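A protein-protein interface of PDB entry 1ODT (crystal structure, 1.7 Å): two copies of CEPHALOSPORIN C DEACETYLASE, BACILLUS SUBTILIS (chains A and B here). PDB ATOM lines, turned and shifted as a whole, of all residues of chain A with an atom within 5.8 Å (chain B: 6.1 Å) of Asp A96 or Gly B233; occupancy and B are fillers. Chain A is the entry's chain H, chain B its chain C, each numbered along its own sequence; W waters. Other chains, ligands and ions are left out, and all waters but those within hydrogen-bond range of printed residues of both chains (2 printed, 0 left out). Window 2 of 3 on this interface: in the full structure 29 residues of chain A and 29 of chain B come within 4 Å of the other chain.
O of Phe B228 sits at hydrogen-bond distance from ND2 of Asn B232, at 3.0 Å.
NE1 of Trp A72 sits at hydrogen-bond distance from O of Asp A96 (2.9 Å).
The side-chain hydroxyl (OG) of Ser A94 lies close to the backbone NH (N) of Gly A97 (3.3 Å).
OE1 of Glu A98 lies within hydrogen-bond range of OG of Ser A94, at 2.5 Å.
The side-chain amide nitrogen (NE2) of Gln A121 sits at hydrogen-bond distance from the backbone carbonyl oxygen (O) of Ser A94, at 3.2 Å.
N of Tyr A95 sits at hydrogen-bond distance from OE2 of Glu A98, 2.7 Å away.
Asp A96 touches three residues of chain B.
Of chain A, only Asp A96 (2.9 Å) comes within 4 Å of Gly B233.
Printed residues of chain B within 4 Å of Ser A94: Arg B231.
Of the printed residues of chain B, Gln A121 touches Arg B231 and Asn B232.
The nearest printed residue of chain A that does not touch Arg B230 is Asp A96 (4.7 Å).
Hydrophobic or aromatic side chains of chain A within 4 Å of the printed part of chain B: Tyr A95.
Of the 10 printed residues of chain B, 4 touch a printed residue of chain A.
Among the printed residues, no Asp or Glu carboxylate lies within 4 Å of a Lys or Arg side-chain nitrogen of the other chain.
The guanidinium group (NH2) of Arg B231 is in hydrogen-bond range of the side-chain hydroxyl (OH) of Tyr A95.
The backbone carbonyl oxygen of Arg B231 sits at hydrogen-bond distance from the backbone NH of Asp A96, 2.8 Å away.
O of Arg B231 is in hydrogen-bond range of NE2 of Gln A121 (3.1 Å).
The backbone NH (N) of Gly B233 sits at hydrogen-bond distance from the side-chain carboxylate (OD2) of Asp A96.
No position is printed for both chains.
Water W1 lies within hydrogen-bond range of OD1 of Asp A96 (2.7 Å), N of Ser B234 (3.0 Å) and N of Gly B233 (3.1 Å).
Water W2 bridges the backbone carbonyl oxygen of Arg B230 (2.7 Å) and the side-chain carboxylate of Asp A96 (2.9 Å).
Ser A94 touches Arg B231 (O to CG, 3.4 Å).
Tyr A95 touches Arg B230 (CD2 to O, 3.3 Å).
Asp A96 touches Asn B232.
Gln A121 touches Asn B232 (OE1 to OD1, 3.7 Å).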
ATOM      1  N   ARG A  58      -3.491  -0.183  19.102  1.00  0.00           N
ATOM      2  CA  ARG A  58      -2.790   0.306  20.280  1.00  0.00           C
ATOM      3  C   ARG A  58      -3.181   1.783  20.467  1.00  0.00           C
ATOM      4  O   ARG A  58      -2.938   2.608  19.596  1.00  0.00           O
ATOM      5  CB  ARG A  58      -1.284   0.126  20.093  1.00  0.00           C
ATOM      6  CG  ARG A  58      -0.496   0.373  21.360  1.00  0.00           C
ATOM      7  CD  ARG A  58      -0.763  -0.668  22.436  1.00  0.00           C
ATOM      8  NE  ARG A  58       0.381  -0.757  23.331  1.00  0.00           N
ATOM      9  CZ  ARG A  58       0.503  -1.652  24.305  1.00  0.00           C
ATOM     10  NH1 ARG A  58      -0.443  -2.552  24.508  1.00  0.00           N
ATOM     11  NH2 ARG A  58       1.582  -1.644  25.074  1.00  0.00           N
ATOM     12  N   TRP A  72      -4.494  -1.822  24.728  1.00  0.00           N
ATOM     13  CA  TRP A  72      -5.228  -2.308  23.597  1.00  0.00           C
ATOM     14  C   TRP A  72      -6.658  -1.785  23.575  1.00  0.00           C
ATOM     15  O   TRP A  72      -7.328  -1.677  24.583  1.00  0.00           O
ATOM     16  CB  TRP A  72      -5.220  -3.845  23.576  1.00  0.00           C
ATOM     17  CG  TRP A  72      -3.824  -4.471  23.631  1.00  0.00           C
ATOM     18  CD1 TRP A  72      -3.299  -5.167  24.673  1.00  0.00           C
ATOM     19  CD2 TRP A  72      -2.783  -4.401  22.638  1.00  0.00           C
ATOM     20  NE1 TRP A  72      -2.017  -5.575  24.386  1.00  0.00           N
ATOM     21  CE2 TRP A  72      -1.675  -5.119  23.144  1.00  0.00           C
ATOM     22  CE3 TRP A  72      -2.682  -3.836  21.365  1.00  0.00           C
ATOM     23  CZ2 TRP A  72      -0.483  -5.276  22.425  1.00  0.00           C
ATOM     24  CZ3 TRP A  72      -1.507  -4.001  20.643  1.00  0.00           C
ATOM     25  CH2 TRP A  72      -0.418  -4.699  21.182  1.00  0.00           C
ATOM     26  N   SER A  94      -0.927  -7.702  34.683  1.00  0.00           N
ATOM     27  CA  SER A  94      -1.155  -7.607  33.283  1.00  0.00           C
ATOM     28  C   SER A  94      -0.027  -8.283  32.528  1.00  0.00           C
ATOM     29  O   SER A  94       1.158  -8.009  32.774  1.00  0.00           O
ATOM     30  CB  SER A  94      -1.267  -6.155  32.825  1.00  0.00           C
ATOM     31  OG  SER A  94      -1.663  -6.126  31.463  1.00  0.00           O
ATOM     32  N   TYR A  95      -0.394  -9.191  31.646  1.00  0.00           N
ATOM     33  CA  TYR A  95       0.563  -9.920  30.856  1.00  0.00           C
ATOM     34  C   TYR A  95       0.344  -9.516  29.406  1.00  0.00           C
ATOM     35  O   TYR A  95      -0.643  -9.922  28.761  1.00  0.00           O
ATOM     36  CB  TYR A  95       0.357 -11.425  31.017  1.00  0.00           C
ATOM     37  CG  TYR A  95       0.746 -11.947  32.368  1.00  0.00           C
ATOM     38  CD1 TYR A  95       0.030 -11.603  33.496  1.00  0.00           C
ATOM     39  CD2 TYR A  95       1.822 -12.795  32.499  1.00  0.00           C
ATOM     40  CE1 TYR A  95       0.401 -12.091  34.746  1.00  0.00           C
ATOM     41  CE2 TYR A  95       2.189 -13.293  33.724  1.00  0.00           C
ATOM     42  CZ  TYR A  95       1.495 -12.914  34.835  1.00  0.00           C
ATOM     43  OH  TYR A  95       1.879 -13.447  36.030  1.00  0.00           O
ATOM     44  N   ASP A  96       1.262  -8.704  28.889  1.00  0.00           N
ATOM     45  CA  ASP A  96       1.132  -8.093  27.580  1.00  0.00           C
ATOM     46  C   ASP A  96      -0.218  -7.442  27.324  1.00  0.00           C
ATOM     47  O   ASP A  96      -0.723  -7.444  26.198  1.00  0.00           O
ATOM     48  CB  ASP A  96       1.493  -9.101  26.493  1.00  0.00           C
ATOM     49  CG  ASP A  96       2.973  -9.295  26.369  1.00  0.00           C
ATOM     50  OD1 ASP A  96       3.694  -8.309  26.081  1.00  0.00           O
ATOM     51  OD2 ASP A  96       3.512 -10.396  26.549  1.00  0.00           O
ATOM     52  N   GLY A  97      -0.833  -6.914  28.379  1.00  0.00           N
ATOM     53  CA  GLY A  97      -2.023  -6.104  28.239  1.00  0.00           C
ATOM     54  C   GLY A  97      -3.353  -6.778  27.946  1.00  0.00           C
ATOM     55  O   GLY A  97      -4.298  -6.077  27.631  1.00  0.00           O
ATOM     56  N   GLU A  98      -3.438  -8.105  28.099  1.00  0.00           N
ATOM     57  CA  GLU A  98      -4.696  -8.823  27.928  1.00  0.00           C
ATOM     58  C   GLU A  98      -5.332  -8.556  26.560  1.00  0.00           C
ATOM     59  O   GLU A  98      -6.549  -8.368  26.465  1.00  0.00           O
ATOM     60  CB  GLU A  98      -5.666  -8.461  29.053  1.00  0.00           C
ATOM     61  CG  GLU A  98      -5.297  -9.070  30.390  1.00  0.00           C
ATOM     62  CD  GLU A  98      -3.989  -8.531  30.910  1.00  0.00           C
ATOM     63  OE1 GLU A  98      -3.886  -7.283  31.105  1.00  0.00           O
ATOM     64  OE2 GLU A  98      -3.074  -9.348  31.114  1.00  0.00           O
ATOM     65  N   ILE A  99      -4.512  -8.591  25.499  1.00  0.00           N
ATOM     66  CA  ILE A  99      -5.027  -8.278  24.175  1.00  0.00           C
ATOM     67  C   ILE A  99      -6.191  -9.184  23.790  1.00  0.00           C
ATOM     68  O   ILE A  99      -7.180  -8.718  23.215  1.00  0.00           O
ATOM     69  CB  ILE A  99      -3.904  -8.325  23.118  1.00  0.00           C
ATOM     70  CG1 ILE A  99      -4.422  -7.662  21.838  1.00  0.00           C
ATOM     71  CG2 ILE A  99      -3.389  -9.717  22.922  1.00  0.00           C
ATOM     72  CD1 ILE A  99      -3.388  -7.528  20.775  1.00  0.00           C
ATOM     73  N   LEU A 116      -3.606   0.229  30.577  1.00  0.00           N
ATOM     74  CA  LEU A 116      -2.510  -0.409  31.265  1.00  0.00           C
ATOM     75  C   LEU A 116      -1.954   0.563  32.315  1.00  0.00           C
ATOM     76  O   LEU A 116      -1.762   1.759  32.047  1.00  0.00           O
ATOM     77  CB  LEU A 116      -1.465  -0.920  30.241  1.00  0.00           C
ATOM     78  CG  LEU A 116      -2.131  -1.783  29.185  1.00  0.00           C
ATOM     79  CD1 LEU A 116      -1.114  -2.308  28.153  1.00  0.00           C
ATOM     80  CD2 LEU A 116      -2.890  -2.937  29.802  1.00  0.00           C
ATOM     81  N   GLN A 121       2.668  -1.991  33.542  1.00  0.00           N
ATOM     82  CA  GLN A 121       2.622  -2.652  32.257  1.00  0.00           C
ATOM     83  C   GLN A 121       2.466  -1.596  31.161  1.00  0.00           C
ATOM     84  O   GLN A 121       1.492  -0.881  31.136  1.00  0.00           O
ATOM     85  CB  GLN A 121       1.493  -3.674  32.231  1.00  0.00           C
ATOM     86  CG  GLN A 121       1.122  -4.192  30.935  1.00  0.00           C
ATOM     87  CD  GLN A 121       2.208  -4.972  30.285  1.00  0.00           C
ATOM     88  OE1 GLN A 121       2.521  -4.746  29.134  1.00  0.00           O
ATOM     89  NE2 GLN A 121       2.772  -5.918  31.018  1.00  0.00           N
ATOM     90  N   PHE B 228       9.322 -10.202  34.707  1.00  0.00           N
ATOM     91  CA  PHE B 228       9.176  -9.205  33.677  1.00  0.00           C
ATOM     92  C   PHE B 228       9.000  -9.883  32.315  1.00  0.00           C
ATOM     93  O   PHE B 228       8.152  -9.472  31.536  1.00  0.00           O
ATOM     94  CB  PHE B 228      10.367  -8.238  33.706  1.00  0.00           C
ATOM     95  CG  PHE B 228      10.363  -7.240  32.598  1.00  0.00           C
ATOM     96  CD1 PHE B 228       9.620  -6.068  32.698  1.00  0.00           C
ATOM     97  CD2 PHE B 228      11.197  -7.423  31.482  1.00  0.00           C
ATOM     98  CE1 PHE B 228       9.631  -5.133  31.675  1.00  0.00           C
ATOM     99  CE2 PHE B 228      11.198  -6.487  30.441  1.00  0.00           C
ATOM    100  CZ  PHE B 228      10.421  -5.342  30.539  1.00  0.00           C
ATOM    101  N   PHE B 229       9.762 -10.941  32.035  1.00  0.00           N
ATOM    102  CA  PHE B 229       9.634 -11.642  30.779  1.00  0.00           C
ATOM    103  C   PHE B 229       8.295 -12.381  30.666  1.00  0.00           C
ATOM    104  O   PHE B 229       7.742 -12.498  29.577  1.00  0.00           O
ATOM    105  CB  PHE B 229      10.817 -12.596  30.524  1.00  0.00           C
ATOM    106  CG  PHE B 229      12.166 -11.912  30.479  1.00  0.00           C
ATOM    107  CD1 PHE B 229      12.307 -10.646  29.941  1.00  0.00           C
ATOM    108  CD2 PHE B 229      13.294 -12.525  30.985  1.00  0.00           C
ATOM    109  CE1 PHE B 229      13.537 -10.019  29.913  1.00  0.00           C
ATOM    110  CE2 PHE B 229      14.525 -11.891  30.975  1.00  0.00           C
ATOM    111  CZ  PHE B 229      14.653 -10.649  30.431  1.00  0.00           C
ATOM    112  N   ARG B 230       7.742 -12.837  31.788  1.00  0.00           N
ATOM    113  CA  ARG B 230       6.387 -13.377  31.732  1.00  0.00           C
ATOM    114  C   ARG B 230       5.373 -12.325  31.274  1.00  0.00           C
ATOM    115  O   ARG B 230       4.457 -12.654  30.537  1.00  0.00           O
ATOM    116  CB  ARG B 230       5.954 -13.941  33.075  1.00  0.00           C
ATOM    117  CG  ARG B 230       6.685 -15.165  33.469  1.00  0.00           C
ATOM    118  CD  ARG B 230       6.558 -15.498  34.978  1.00  0.00           C
ATOM    119  NE  ARG B 230       5.177 -15.634  35.436  1.00  0.00           N
ATOM    120  CZ  ARG B 230       4.419 -16.690  35.209  1.00  0.00           C
ATOM    121  NH1 ARG B 230       4.905 -17.698  34.523  1.00  0.00           N
ATOM    122  NH2 ARG B 230       3.173 -16.754  35.680  1.00  0.00           N
ATOM    123  N   ARG B 231       5.525 -11.084  31.733  1.00  0.00           N
ATOM    124  CA  ARG B 231       4.521 -10.025  31.501  1.00  0.00           C
ATOM    125  C   ARG B 231       4.782  -9.237  30.205  1.00  0.00           C
ATOM    126  O   ARG B 231       3.914  -8.476  29.757  1.00  0.00           O
ATOM    127  CB  ARG B 231       4.475  -9.023  32.670  1.00  0.00           C
ATOM    128  CG  ARG B 231       3.929  -9.573  33.947  1.00  0.00           C
ATOM    129  CD  ARG B 231       4.419  -8.835  35.197  1.00  0.00           C
ATOM    130  NE  ARG B 231       3.707  -9.334  36.355  1.00  0.00           N
ATOM    131  CZ  ARG B 231       3.903 -10.523  36.905  1.00  0.00           C
ATOM    132  NH1 ARG B 231       4.839 -11.352  36.438  1.00  0.00           N
ATOM    133  NH2 ARG B 231       3.161 -10.903  37.949  1.00  0.00           N
ATOM    134  N   ASN B 232       5.938  -9.472  29.585  1.00  0.00           N
ATOM    135  CA  ASN B 232       6.390  -8.780  28.372  1.00  0.00           C
ATOM    136  C   ASN B 232       7.142  -9.814  27.573  1.00  0.00           C
ATOM    137  O   ASN B 232       8.324  -9.955  27.741  1.00  0.00           O
ATOM    138  CB  ASN B 232       7.322  -7.601  28.746  1.00  0.00           C
ATOM    139  CG  ASN B 232       6.646  -6.584  29.703  1.00  0.00           C
ATOM    140  OD1 ASN B 232       6.067  -5.625  29.266  1.00  0.00           O
ATOM    141  ND2 ASN B 232       6.724  -6.843  31.017  1.00  0.00           N
ATOM    142  N   GLY B 233       6.411 -10.558  26.731  1.00  0.00           N
ATOM    143  CA  GLY B 233       6.834 -11.853  26.232  1.00  0.00           C
ATOM    144  C   GLY B 233       7.567 -11.866  24.914  1.00  0.00           C
ATOM    145  O   GLY B 233       8.035 -12.925  24.435  1.00  0.00           O
ATOM    146  N   SER B 234       7.687 -10.710  24.308  1.00  0.00           N
ATOM    147  CA  SER B 234       8.349 -10.633  23.017  1.00  0.00           C
ATOM    148  C   SER B 234       9.820 -11.091  23.082  1.00  0.00           C
ATOM    149  O   SER B 234      10.546 -10.689  23.976  1.00  0.00           O
ATOM    150  CB  SER B 234       8.238  -9.205  22.498  1.00  0.00           C
ATOM    151  OG  SER B 234       9.395  -8.815  21.830  1.00  0.00           O
ATOM    152  N   PRO B 235      10.245 -11.961  22.173  1.00  0.00           N
ATOM    153  CA  PRO B 235      11.660 -12.401  22.166  1.00  0.00           C
ATOM    154  C   PRO B 235      12.640 -11.206  22.113  1.00  0.00           C
ATOM    155  O   PRO B 235      13.676 -11.226  22.774  1.00  0.00           O
ATOM    156  CB  PRO B 235      11.741 -13.331  20.949  1.00  0.00           C
ATOM    157  CG  PRO B 235      10.344 -13.830  20.751  1.00  0.00           C
ATOM    158  CD  PRO B 235       9.442 -12.687  21.171  1.00  0.00           C
ATOM    159  N   GLU B 236      12.268 -10.147  21.410  1.00  0.00           N
ATOM    160  CA  GLU B 236      13.116  -8.973  21.237  1.00  0.00           C
ATOM    161  C   GLU B 236      13.271  -8.202  22.552  1.00  0.00           C
ATOM    162  O   GLU B 236      14.339  -7.655  22.826  1.00  0.00           O
ATOM    163  CB  GLU B 236      12.570  -8.068  20.101  1.00  0.00           C
ATOM    164  CG  GLU B 236      12.009  -8.839  18.890  1.00  0.00           C
ATOM    165  CD  GLU B 236      10.593  -9.433  19.107  1.00  0.00           C
ATOM    166  OE1 GLU B 236       9.628  -8.669  19.368  1.00  0.00           O
ATOM    167  OE2 GLU B 236      10.425 -10.670  19.018  1.00  0.00           O
ATOM    168  N   THR B 237      12.202  -8.154  23.368  1.00  0.00           N
ATOM    169  CA  THR B 237      12.247  -7.547  24.694  1.00  0.00           C
ATOM    170  C   THR B 237      13.273  -8.262  25.584  1.00  0.00           C
ATOM    171  O   THR B 237      14.100  -7.638  26.257  1.00  0.00           O
ATOM    172  CB  THR B 237      10.849  -7.576  25.307  1.00  0.00           C
ATOM    173  OG1 THR B 237      10.017  -6.679  24.551  1.00  0.00           O
ATOM    174  CG2 THR B 237      10.820  -7.057  26.728  1.00  0.00           C
HETATM  175  O   HOH W   1       5.981  -8.213  24.679  1.00  0.00           O
HETATM  176  O   HOH W   2       2.789 -12.457  28.382  1.00  0.00           O
